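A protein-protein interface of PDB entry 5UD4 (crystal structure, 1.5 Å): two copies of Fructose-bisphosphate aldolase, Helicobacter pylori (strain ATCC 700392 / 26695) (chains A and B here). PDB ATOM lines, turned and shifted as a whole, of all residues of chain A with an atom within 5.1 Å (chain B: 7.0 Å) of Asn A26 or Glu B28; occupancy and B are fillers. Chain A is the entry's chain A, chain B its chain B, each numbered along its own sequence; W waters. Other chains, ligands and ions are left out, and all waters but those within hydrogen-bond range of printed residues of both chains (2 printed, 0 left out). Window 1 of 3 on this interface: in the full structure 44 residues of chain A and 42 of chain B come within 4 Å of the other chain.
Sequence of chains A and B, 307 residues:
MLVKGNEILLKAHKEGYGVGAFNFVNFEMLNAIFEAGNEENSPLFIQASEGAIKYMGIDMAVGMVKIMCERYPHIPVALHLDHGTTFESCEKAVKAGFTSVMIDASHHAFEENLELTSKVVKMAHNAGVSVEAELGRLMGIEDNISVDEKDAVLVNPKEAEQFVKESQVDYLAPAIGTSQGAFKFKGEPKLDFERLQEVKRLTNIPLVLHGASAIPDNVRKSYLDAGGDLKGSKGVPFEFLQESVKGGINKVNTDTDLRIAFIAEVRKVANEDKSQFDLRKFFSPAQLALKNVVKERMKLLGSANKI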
ATOM      1  N   PHE A  24      27.521 -22.917  -4.737  1.00  0.00           N
ATOM      2  CA  PHE A  24      27.731 -23.642  -5.981  1.00  0.00           C
ATOM      3  C   PHE A  24      27.132 -22.851  -7.130  1.00  0.00           C
ATOM      4  O   PHE A  24      26.196 -22.075  -6.938  1.00  0.00           O
ATOM      5  CB  PHE A  24      27.125 -25.051  -5.935  1.00  0.00           C
ATOM      6  CG  PHE A  24      25.631 -25.114  -6.085  1.00  0.00           C
ATOM      7  CD1 PHE A  24      24.794 -24.732  -5.050  1.00  0.00           C
ATOM      8  CD2 PHE A  24      25.058 -25.654  -7.227  1.00  0.00           C
ATOM      9  CE1 PHE A  24      23.420 -24.827  -5.177  1.00  0.00           C
ATOM     10  CE2 PHE A  24      23.689 -25.773  -7.343  1.00  0.00           C
ATOM     11  CZ  PHE A  24      22.869 -25.337  -6.332  1.00  0.00           C
ATOM     12  N   VAL A  25      27.687 -23.066  -8.330  1.00  0.00           N
ATOM     13  CA  VAL A  25      27.107 -22.502  -9.548  1.00  0.00           C
ATOM     14  C   VAL A  25      26.857 -23.566 -10.601  1.00  0.00           C
ATOM     15  O   VAL A  25      26.335 -23.240 -11.666  1.00  0.00           O
ATOM     16  CB  VAL A  25      27.972 -21.389 -10.170  1.00  0.00           C
ATOM     17  CG1 VAL A  25      28.298 -20.330  -9.144  1.00  0.00           C
ATOM     18  CG2 VAL A  25      29.238 -21.939 -10.795  1.00  0.00           C
ATOM     19  N   ASN A  26      27.267 -24.810 -10.368  1.00  0.00           N
ATOM     20  CA  ASN A  26      27.054 -25.831 -11.400  1.00  0.00           C
ATOM     21  C   ASN A  26      27.208 -27.229 -10.798  1.00  0.00           C
ATOM     22  O   ASN A  26      27.322 -27.396  -9.581  1.00  0.00           O
ATOM     23  CB  ASN A  26      27.981 -25.593 -12.597  1.00  0.00           C
ATOM     24  CG  ASN A  26      29.443 -25.871 -12.303  1.00  0.00           C
ATOM     25  OD1 ASN A  26      29.812 -26.426 -11.255  1.00  0.00           O
ATOM     26  ND2 ASN A  26      30.302 -25.473 -13.248  1.00  0.00           N
ATOM     27  N   PHE A  27      27.174 -28.252 -11.664  1.00  0.00           N
ATOM     28  CA  PHE A  27      27.189 -29.634 -11.183  1.00  0.00           C
ATOM     29  C   PHE A  27      28.512 -29.981 -10.510  1.00  0.00           C
ATOM     30  O   PHE A  27      28.532 -30.631  -9.459  1.00  0.00           O
ATOM     31  CB  PHE A  27      26.929 -30.622 -12.331  1.00  0.00           C
ATOM     32  CG  PHE A  27      27.342 -32.024 -12.011  1.00  0.00           C
ATOM     33  CD1 PHE A  27      26.608 -32.783 -11.124  1.00  0.00           C
ATOM     34  CD2 PHE A  27      28.483 -32.566 -12.570  1.00  0.00           C
ATOM     35  CE1 PHE A  27      27.003 -34.069 -10.791  1.00  0.00           C
ATOM     36  CE2 PHE A  27      28.889 -33.857 -12.256  1.00  0.00           C
ATOM     37  CZ  PHE A  27      28.147 -34.610 -11.366  1.00  0.00           C
ATOM     38  N   GLU A  28      29.629 -29.587 -11.115  1.00  0.00           N
ATOM     39  CA  GLU A  28      30.928 -29.980 -10.581  1.00  0.00           C
ATOM     40  C   GLU A  28      31.122 -29.469  -9.165  1.00  0.00           C
ATOM     41  O   GLU A  28      31.619 -30.199  -8.304  1.00  0.00           O
ATOM     42  CB  GLU A  28      32.053 -29.481 -11.481  1.00  0.00           C
ATOM     43  CG  GLU A  28      32.286 -30.358 -12.682  1.00  0.00           C
ATOM     44  CD  GLU A  28      31.374 -30.067 -13.834  1.00  0.00           C
ATOM     45  OE1 GLU A  28      30.567 -29.107 -13.763  1.00  0.00           O
ATOM     46  OE2 GLU A  28      31.490 -30.810 -14.828  1.00  0.00           O
ATOM     47  N   MET A  29      30.758 -28.209  -8.905  1.00  0.00           N
ATOM     48  CA  MET A  29      30.896 -27.689  -7.549  1.00  0.00           C
ATOM     49  C   MET A  29      30.009 -28.469  -6.598  1.00  0.00           C
ATOM     50  O   MET A  29      30.445 -28.887  -5.519  1.00  0.00           O
ATOM     51  CB  MET A  29      30.562 -26.195  -7.502  1.00  0.00           C
ATOM     52  CG  MET A  29      31.551 -25.299  -8.223  1.00  0.00           C
ATOM     53  SD  MET A  29      31.170 -23.560  -7.925  1.00  0.00           S
ATOM     54  CE  MET A  29      31.844 -23.308  -6.290  1.00  0.00           C
ATOM     55  N   LEU A  30      28.759 -28.701  -7.005  1.00  0.00           N
ATOM     56  CA  LEU A  30      27.799 -29.383  -6.153  1.00  0.00           C
ATOM     57  C   LEU A  30      28.251 -30.802  -5.848  1.00  0.00           C
ATOM     58  O   LEU A  30      28.167 -31.257  -4.702  1.00  0.00           O
ATOM     59  CB  LEU A  30      26.435 -29.372  -6.843  1.00  0.00           C
ATOM     60  CG  LEU A  30      25.262 -29.860  -6.020  1.00  0.00           C
ATOM     61  CD1 LEU A  30      25.082 -28.978  -4.808  1.00  0.00           C
ATOM     62  CD2 LEU A  30      23.996 -29.910  -6.840  1.00  0.00           C
ATOM     63  N   TYR A  55      22.298 -17.980 -13.424  1.00  0.00           N
ATOM     64  CA  TYR A  55      23.170 -18.753 -14.304  1.00  0.00           C
ATOM     65  C   TYR A  55      22.615 -20.155 -14.539  1.00  0.00           C
ATOM     66  O   TYR A  55      22.547 -20.622 -15.682  1.00  0.00           O
ATOM     67  CB  TYR A  55      24.579 -18.785 -13.700  1.00  0.00           C
ATOM     68  CG  TYR A  55      25.585 -19.642 -14.420  1.00  0.00           C
ATOM     69  CD1 TYR A  55      26.291 -19.144 -15.491  1.00  0.00           C
ATOM     70  CD2 TYR A  55      25.874 -20.927 -13.981  1.00  0.00           C
ATOM     71  CE1 TYR A  55      27.221 -19.911 -16.141  1.00  0.00           C
ATOM     72  CE2 TYR A  55      26.793 -21.694 -14.617  1.00  0.00           C
ATOM     73  CZ  TYR A  55      27.489 -21.174 -15.689  1.00  0.00           C
ATOM     74  OH  TYR A  55      28.419 -21.931 -16.366  1.00  0.00           O
ATOM     75  N   MET A  56      22.180 -20.826 -13.473  1.00  0.00           N
ATOM     76  CA  MET A  56      21.650 -22.186 -13.596  1.00  0.00           C
ATOM     77  C   MET A  56      20.195 -22.214 -14.029  1.00  0.00           C
ATOM     78  O   MET A  56      19.767 -23.158 -14.715  1.00  0.00           O
ATOM     79  CB  MET A  56      21.752 -22.915 -12.260  1.00  0.00           C
ATOM     80  CG  MET A  56      23.156 -23.320 -11.859  1.00  0.00           C
ATOM     81  SD  MET A  56      23.228 -24.140 -10.258  1.00  0.00           S
ATOM     82  CE  MET A  56      23.250 -22.716  -9.183  1.00  0.00           C
ATOM     83  N   MET A  64      19.026 -30.098  -9.247  1.00  0.00           N
ATOM     84  CA  MET A  64      20.291 -30.800  -9.050  1.00  0.00           C
ATOM     85  C   MET A  64      20.497 -31.134  -7.586  1.00  0.00           C
ATOM     86  O   MET A  64      20.979 -32.220  -7.257  1.00  0.00           O
ATOM     87  CB  MET A  64      21.481 -29.989  -9.561  1.00  0.00           C
ATOM     88  CG  MET A  64      21.594 -29.873 -11.096  1.00  0.00           C
ATOM     89  SD  MET A  64      23.191 -29.244 -11.707  1.00  0.00           S
ATOM     90  CE  MET A  64      23.254 -27.703 -10.829  1.00  0.00           C
ATOM     91  N   PHE B  24      26.858 -34.624 -24.103  1.00  0.00           N
ATOM     92  CA  PHE B  24      27.087 -33.731 -22.973  1.00  0.00           C
ATOM     93  C   PHE B  24      27.744 -34.492 -21.829  1.00  0.00           C
ATOM     94  O   PHE B  24      27.596 -35.716 -21.707  1.00  0.00           O
ATOM     95  CB  PHE B  24      25.793 -33.067 -22.498  1.00  0.00           C
ATOM     96  CG  PHE B  24      24.880 -33.946 -21.697  1.00  0.00           C
ATOM     97  CD1 PHE B  24      24.161 -34.954 -22.309  1.00  0.00           C
ATOM     98  CD2 PHE B  24      24.669 -33.717 -20.342  1.00  0.00           C
ATOM     99  CE1 PHE B  24      23.283 -35.760 -21.576  1.00  0.00           C
ATOM    100  CE2 PHE B  24      23.780 -34.508 -19.611  1.00  0.00           C
ATOM    101  CZ  PHE B  24      23.094 -35.534 -20.231  1.00  0.00           C
ATOM    102  N   VAL B  25      28.462 -33.743 -20.976  1.00  0.00           N
ATOM    103  CA  VAL B  25      29.057 -34.302 -19.761  1.00  0.00           C
ATOM    104  C   VAL B  25      28.675 -33.503 -18.518  1.00  0.00           C
ATOM    105  O   VAL B  25      28.983 -33.933 -17.405  1.00  0.00           O
ATOM    106  CB  VAL B  25      30.596 -34.418 -19.854  1.00  0.00           C
ATOM    107  CG1 VAL B  25      30.986 -35.228 -21.074  1.00  0.00           C
ATOM    108  CG2 VAL B  25      31.305 -33.041 -19.792  1.00  0.00           C
ATOM    109  N   ASN B  26      28.018 -32.356 -18.675  1.00  0.00           N
ATOM    110  CA  ASN B  26      27.663 -31.566 -17.492  1.00  0.00           C
ATOM    111  C   ASN B  26      26.559 -30.561 -17.834  1.00  0.00           C
ATOM    112  O   ASN B  26      25.975 -30.596 -18.921  1.00  0.00           O
ATOM    113  CB  ASN B  26      28.916 -30.897 -16.902  1.00  0.00           C
ATOM    114  CG  ASN B  26      29.511 -29.818 -17.798  1.00  0.00           C
ATOM    115  OD1 ASN B  26      28.926 -29.392 -18.808  1.00  0.00           O
ATOM    116  ND2 ASN B  26      30.699 -29.374 -17.431  1.00  0.00           N
ATOM    117  N   PHE B  27      26.264 -29.660 -16.888  1.00  0.00           N
ATOM    118  CA  PHE B  27      25.166 -28.718 -17.060  1.00  0.00           C
ATOM    119  C   PHE B  27      25.441 -27.735 -18.195  1.00  0.00           C
ATOM    120  O   PHE B  27      24.563 -27.449 -19.010  1.00  0.00           O
ATOM    121  CB  PHE B  27      24.919 -27.931 -15.761  1.00  0.00           C
ATOM    122  CG  PHE B  27      24.105 -26.677 -15.976  1.00  0.00           C
ATOM    123  CD1 PHE B  27      22.765 -26.756 -16.304  1.00  0.00           C
ATOM    124  CD2 PHE B  27      24.695 -25.422 -15.936  1.00  0.00           C
ATOM    125  CE1 PHE B  27      22.038 -25.619 -16.553  1.00  0.00           C
ATOM    126  CE2 PHE B  27      23.945 -24.276 -16.186  1.00  0.00           C
ATOM    127  CZ  PHE B  27      22.642 -24.373 -16.501  1.00  0.00           C
ATOM    128  N   GLU B  28      26.648 -27.182 -18.244  1.00  0.00           N
ATOM    129  CA  GLU B  28      26.934 -26.141 -19.219  1.00  0.00           C
ATOM    130  C   GLU B  28      26.772 -26.660 -20.643  1.00  0.00           C
ATOM    131  O   GLU B  28      26.209 -25.973 -21.503  1.00  0.00           O
ATOM    132  CB  GLU B  28      28.337 -25.591 -18.999  1.00  0.00           C
ATOM    133  CG  GLU B  28      28.424 -24.568 -17.889  1.00  0.00           C
ATOM    134  CD  GLU B  28      28.669 -25.170 -16.533  1.00  0.00           C
ATOM    135  OE1 GLU B  28      28.763 -26.417 -16.397  1.00  0.00           O
ATOM    136  OE2 GLU B  28      28.786 -24.378 -15.591  1.00  0.00           O
ATOM    137  N   MET B  29      27.249 -27.873 -20.922  1.00  0.00           N
ATOM    138  CA  MET B  29      27.064 -28.405 -22.274  1.00  0.00           C
ATOM    139  C   MET B  29      25.584 -28.567 -22.575  1.00  0.00           C
ATOM    140  O   MET B  29      25.103 -28.188 -23.652  1.00  0.00           O
ATOM    141  CB  MET B  29      27.786 -29.742 -22.425  1.00  0.00           C
ATOM    142  CG  MET B  29      29.307 -29.648 -22.393  1.00  0.00           C
ATOM    143  SD  MET B  29      30.136 -31.199 -22.830  1.00  0.00           S
ATOM    144  CE  MET B  29      29.946 -31.276 -24.606  1.00  0.00           C
ATOM    145  N   LEU B  30      24.851 -29.141 -21.626  1.00  0.00           N
ATOM    146  CA  LEU B  30      23.434 -29.410 -21.815  1.00  0.00           C
ATOM    147  C   LEU B  30      22.656 -28.124 -22.038  1.00  0.00           C
ATOM    148  O   LEU B  30      21.795 -28.049 -22.922  1.00  0.00           O
ATOM    149  CB  LEU B  30      22.904 -30.157 -20.601  1.00  0.00           C
ATOM    150  CG  LEU B  30      21.504 -30.710 -20.698  1.00  0.00           C
ATOM    151  CD1 LEU B  30      21.439 -31.798 -21.743  1.00  0.00           C
ATOM    152  CD2 LEU B  30      21.086 -31.254 -19.346  1.00  0.00           C
ATOM    153  N   ASN B  31      22.932 -27.108 -21.229  1.00  0.00           N
ATOM    154  CA  ASN B  31      22.205 -25.854 -21.354  1.00  0.00           C
ATOM    155  C   ASN B  31      22.420 -25.234 -22.727  1.00  0.00           C
ATOM    156  O   ASN B  31      21.473 -24.751 -23.355  1.00  0.00           O
ATOM    157  CB  ASN B  31      22.650 -24.889 -20.263  1.00  0.00           C
ATOM    158  CG  ASN B  31      21.746 -23.684 -20.162  1.00  0.00           C
ATOM    159  OD1 ASN B  31      20.530 -23.819 -20.181  1.00  0.00           O
ATOM    160  ND2 ASN B  31      22.337 -22.499 -20.092  1.00  0.00           N
ATOM    161  N   ALA B  32      23.661 -25.248 -23.211  1.00  0.00           N
ATOM    162  CA  ALA B  32      23.963 -24.654 -24.505  1.00  0.00           C
ATOM    163  C   ALA B  32      23.277 -25.409 -25.635  1.00  0.00           C
ATOM    164  O   ALA B  32      22.764 -24.802 -26.588  1.00  0.00           O
ATOM    165  CB  ALA B  32      25.476 -24.605 -24.702  1.00  0.00           C
ATOM    166  N   ILE B  33      23.224 -26.733 -25.538  1.00  0.00           N
ATOM    167  CA  ILE B  33      22.557 -27.530 -26.572  1.00  0.00           C
ATOM    168  C   ILE B  33      21.071 -27.196 -26.628  1.00  0.00           C
ATOM    169  O   ILE B  33      20.499 -27.006 -27.710  1.00  0.00           O
ATOM    170  CB  ILE B  33      22.802 -29.026 -26.314  1.00  0.00           C
ATOM    171  CG1 ILE B  33      24.274 -29.383 -26.551  1.00  0.00           C
ATOM    172  CG2 ILE B  33      21.927 -29.864 -27.190  1.00  0.00           C
ATOM    173  CD1 ILE B  33      24.672 -30.722 -25.911  1.00  0.00           C
ATOM    174  N   MET B  64      18.979 -34.001 -15.030  1.00  0.00           N
ATOM    175  CA  MET B  64      19.205 -32.699 -15.646  1.00  0.00           C
ATOM    176  C   MET B  64      18.445 -32.585 -16.955  1.00  0.00           C
ATOM    177  O   MET B  64      17.881 -31.526 -17.266  1.00  0.00           O
ATOM    178  CB  MET B  64      20.696 -32.444 -15.877  1.00  0.00           C
ATOM    179  CG  MET B  64      21.494 -32.126 -14.609  1.00  0.00           C
ATOM    180  SD  MET B  64      23.147 -31.462 -14.934  1.00  0.00           S
ATOM    181  CE  MET B  64      23.821 -32.707 -15.987  1.00  0.00           C
ATOM    182  N   PHE B 262      34.073 -25.045 -26.710  1.00  0.00           N
ATOM    183  CA  PHE B 262      33.915 -24.748 -25.292  1.00  0.00           C
ATOM    184  C   PHE B 262      35.265 -24.445 -24.644  1.00  0.00           C
ATOM    185  O   PHE B 262      35.434 -23.420 -23.986  1.00  0.00           O
ATOM    186  CB  PHE B 262      33.243 -25.940 -24.618  1.00  0.00           C
ATOM    187  CG  PHE B 262      32.815 -25.692 -23.207  1.00  0.00           C
ATOM    188  CD1 PHE B 262      31.501 -25.333 -22.919  1.00  0.00           C
ATOM    189  CD2 PHE B 262      33.714 -25.829 -22.162  1.00  0.00           C
ATOM    190  CE1 PHE B 262      31.105 -25.127 -21.616  1.00  0.00           C
ATOM    191  CE2 PHE B 262      33.302 -25.624 -20.844  1.00  0.00           C
ATOM    192  CZ  PHE B 262      32.011 -25.276 -20.581  1.00  0.00           C
ATOM    193  N   LEU B 279      33.780 -19.157 -11.791  1.00  0.00           N
ATOM    194  CA  LEU B 279      33.542 -20.179 -12.813  1.00  0.00           C
ATOM    195  C   LEU B 279      32.628 -19.665 -13.921  1.00  0.00           C
ATOM    196  O   LEU B 279      32.807 -20.027 -15.093  1.00  0.00           O
ATOM    197  CB  LEU B 279      32.949 -21.454 -12.191  1.00  0.00           C
ATOM    198  CG  LEU B 279      33.882 -22.477 -11.524  1.00  0.00           C
ATOM    199  CD1 LEU B 279      34.581 -21.884 -10.299  1.00  0.00           C
ATOM    200  CD2 LEU B 279      33.094 -23.699 -11.117  1.00  0.00           C
ATOM    201  N   ARG B 280      31.663 -18.808 -13.584  1.00  0.00           N
ATOM    202  CA  ARG B 280      30.727 -18.306 -14.582  1.00  0.00           C
ATOM    203  C   ARG B 280      31.410 -17.462 -15.646  1.00  0.00           C
ATOM    204  O   ARG B 280      30.945 -17.413 -16.794  1.00  0.00           O
ATOM    205  CB  ARG B 280      29.634 -17.495 -13.897  1.00  0.00           C
ATOM    206  CG  ARG B 280      28.776 -18.325 -12.969  1.00  0.00           C
ATOM    207  CD  ARG B 280      28.014 -17.467 -11.979  1.00  0.00           C
ATOM    208  NE  ARG B 280      28.943 -16.773 -11.074  1.00  0.00           N
ATOM    209  CZ  ARG B 280      28.638 -16.304  -9.864  1.00  0.00           C
ATOM    210  NH1 ARG B 280      27.419 -16.429  -9.368  1.00  0.00           N
ATOM    211  NH2 ARG B 280      29.566 -15.697  -9.148  1.00  0.00           N
ATOM    212  N   PHE B 283      32.736 -20.055 -18.054  1.00  0.00           N
ATOM    213  CA  PHE B 283      31.812 -20.964 -18.722  1.00  0.00           C
ATOM    214  C   PHE B 283      30.665 -20.274 -19.451  1.00  0.00           C
ATOM    215  O   PHE B 283      30.025 -20.917 -20.296  1.00  0.00           O
ATOM    216  CB  PHE B 283      31.284 -21.976 -17.717  1.00  0.00           C
ATOM    217  CG  PHE B 283      32.379 -22.771 -17.036  1.00  0.00           C
ATOM    218  CD1 PHE B 283      33.583 -23.027 -17.687  1.00  0.00           C
ATOM    219  CD2 PHE B 283      32.219 -23.216 -15.737  1.00  0.00           C
ATOM    220  CE1 PHE B 283      34.584 -23.729 -17.062  1.00  0.00           C
ATOM    221  CE2 PHE B 283      33.217 -23.917 -15.096  1.00  0.00           C
ATOM    222  CZ  PHE B 283      34.402 -24.178 -15.753  1.00  0.00           C
ATOM    223  N   SER B 284      30.377 -18.992 -19.174  1.00  0.00           N
ATOM    224  CA  SER B 284      29.373 -18.309 -19.988  1.00  0.00           C
ATOM    225  C   SER B 284      29.848 -18.112 -21.424  1.00  0.00           C
ATOM    226  O   SER B 284      29.098 -18.463 -22.357  1.00  0.00           O
ATOM    227  CB  SER B 284      28.971 -16.990 -19.333  1.00  0.00           C
ATOM    228  OG  SER B 284      28.200 -17.257 -18.169  1.00  0.00           O
ATOM    229  N   ALA B 286      32.083 -19.895 -22.888  1.00  0.00           N
ATOM    230  CA  ALA B 286      32.232 -21.266 -23.362  1.00  0.00           C
ATOM    231  C   ALA B 286      30.901 -21.840 -23.845  1.00  0.00           C
ATOM    232  O   ALA B 286      30.832 -22.455 -24.923  1.00  0.00           O
ATOM    233  CB  ALA B 286      32.826 -22.119 -22.253  1.00  0.00           C
ATOM    234  N   GLN B 287      29.842 -21.675 -23.043  1.00  0.00           N
ATOM    235  CA  GLN B 287      28.483 -22.026 -23.469  1.00  0.00           C
ATOM    236  C   GLN B 287      28.106 -21.348 -24.786  1.00  0.00           C
ATOM    237  O   GLN B 287      27.538 -21.976 -25.681  1.00  0.00           O
ATOM    238  CB  GLN B 287      27.457 -21.646 -22.400  1.00  0.00           C
ATOM    239  CG  GLN B 287      27.388 -22.581 -21.218  1.00  0.00           C
ATOM    240  CD  GLN B 287      26.208 -22.226 -20.320  1.00  0.00           C
ATOM    241  OE1 GLN B 287      25.057 -22.327 -20.734  1.00  0.00           O
ATOM    242  NE2 GLN B 287      26.496 -21.795 -19.096  1.00  0.00           N
ATOM    243  N   LEU B 290      29.786 -22.998 -27.705  1.00  0.00           N
ATOM    244  CA  LEU B 290      29.201 -24.311 -27.954  1.00  0.00           C
ATOM    245  C   LEU B 290      27.823 -24.165 -28.581  1.00  0.00           C
ATOM    246  O   LEU B 290      27.497 -24.830 -29.575  1.00  0.00           O
ATOM    247  CB  LEU B 290      29.150 -25.099 -26.647  1.00  0.00           C
ATOM    248  CG  LEU B 290      28.852 -26.596 -26.744  1.00  0.00           C
ATOM    249  CD1 LEU B 290      29.354 -27.301 -25.480  1.00  0.00           C
ATOM    250  CD2 LEU B 290      27.358 -26.866 -26.945  1.00  0.00           C
HETATM  251  O   HOH W   1      28.089 -28.382 -14.667  1.00  0.00           O
HETATM  252  O   HOH W   2      24.160 -20.348 -18.045  1.00  0.00           O
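Water W1 lies within hydrogen-bond range of the side-chain carboxylate (OE1) of Glu B28 (2.7 Å), the side-chain carboxylate (OE1) of Glu A28 (2.7 Å), the backbone NH (N) of Phe A27 (3.1 Å) and the backbone NH (N) of Phe B27 (3.1 Å).
Water W2 lies within hydrogen-bond range of the backbone carbonyl oxygen of Tyr A55 (2.9 Å), the side-chain amide nitrogen of Gln B287 (2.9 Å) and the side-chain amide nitrogen of Asn B31 (3.5 Å).
Among the printed residues, merely in contact across the chains: Val A25 with Leu B279 (3.99 Å), Asn A26 with Leu B279 (3.9 Å), Asn A26 with Phe B283 (3.8 Å), Met A29 with Leu B279 (3.6 Å), Tyr A55 with Phe B27 (3.8 Å), Tyr A55 with Arg B280 (3.6 Å), Tyr A55 with Phe B283 (3.2 Å), Tyr A55 with Ser B284 (3.5 Å), Met A56 with Phe B27 (3.6 Å) and Met A64 with Met B64 (3.9 Å).
Asn A26 touches Glu B28, and with the chains exchanged Glu A28 touches Asn B26.
Met A64 touches its own counterpart, Met B64.
Positions printed for both chains: 24, 25, 26, 27, 28, 29, 30 and 64.
Of the 10 printed residues of chain A, 7 touch a printed residue of chain B.
Of the 19 printed residues of chain B, 9 touch a printed residue of chain A.
Among the printed residues, 14 pairs touch across the chains.
OD1 of Asn A26 lies within hydrogen-bond range of N of Met A29, at 3.1 Å.
The side-chain amide oxygen of Gln B287 is in hydrogen-bond range of the side-chain amide nitrogen of Asn B31 (2.8 Å).
The backbone carbonyl oxygen (O) of Arg B280 lies within hydrogen-bond range of the side-chain hydroxyl (OG) of Ser B284 (3.1 Å).
The backbone NH (N) of Val A25 is in hydrogen-bond range of the side-chain sulfur (SD) of Met A29 (3.5 Å).
OD1 of Asn B26 is in hydrogen-bond range of N of Met B29 (3.1 Å).
The side-chain amide oxygen (OD1) of Asn A26 sits at hydrogen-bond distance from the backbone NH (N) of Glu A28, 3.2 Å away.
Asn A26 touches just these residues of chain B: Glu B28, Leu B279 and Phe B283.
Leu A30 touches none of the printed residues of chain B.
Printed residues of chain B within 4 Å of Tyr A55: Phe B27, Glu B28, Arg B280, Phe B283, Ser B284 and Gln B287.
Printed residues of chain B within 4 Å of Met A56: Phe B27.
Printed residues of chain B within 4 Å of Met A64: Met B64.
Glu B28 touches just these residues of chain A: Asn A26 and Tyr A55.
Ile B33 touches none of the printed residues of chain A.
The nearest residue of chain B that does not touch Asn A26 is Phe B27 (4.7 Å).
The nearest residue of chain A that does not touch Glu B28 is Glu A28 (4.2 Å).
OH of Tyr A55 is in hydrogen-bond range of OE2 of Glu B28.
The side-chain amide nitrogen (NE2) of Gln B287 is in hydrogen-bond range of the side-chain hydroxyl (OH) of Tyr A55 (3.3 Å).
ND2 of Asn A26 lies within hydrogen-bond range of OE2 of Glu B28 (3.0 Å).
The side-chain carboxylate (OE2) of Glu A28 is in hydrogen-bond range of the side-chain amide nitrogen (ND2) of Asn B26, 3.1 Å away.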
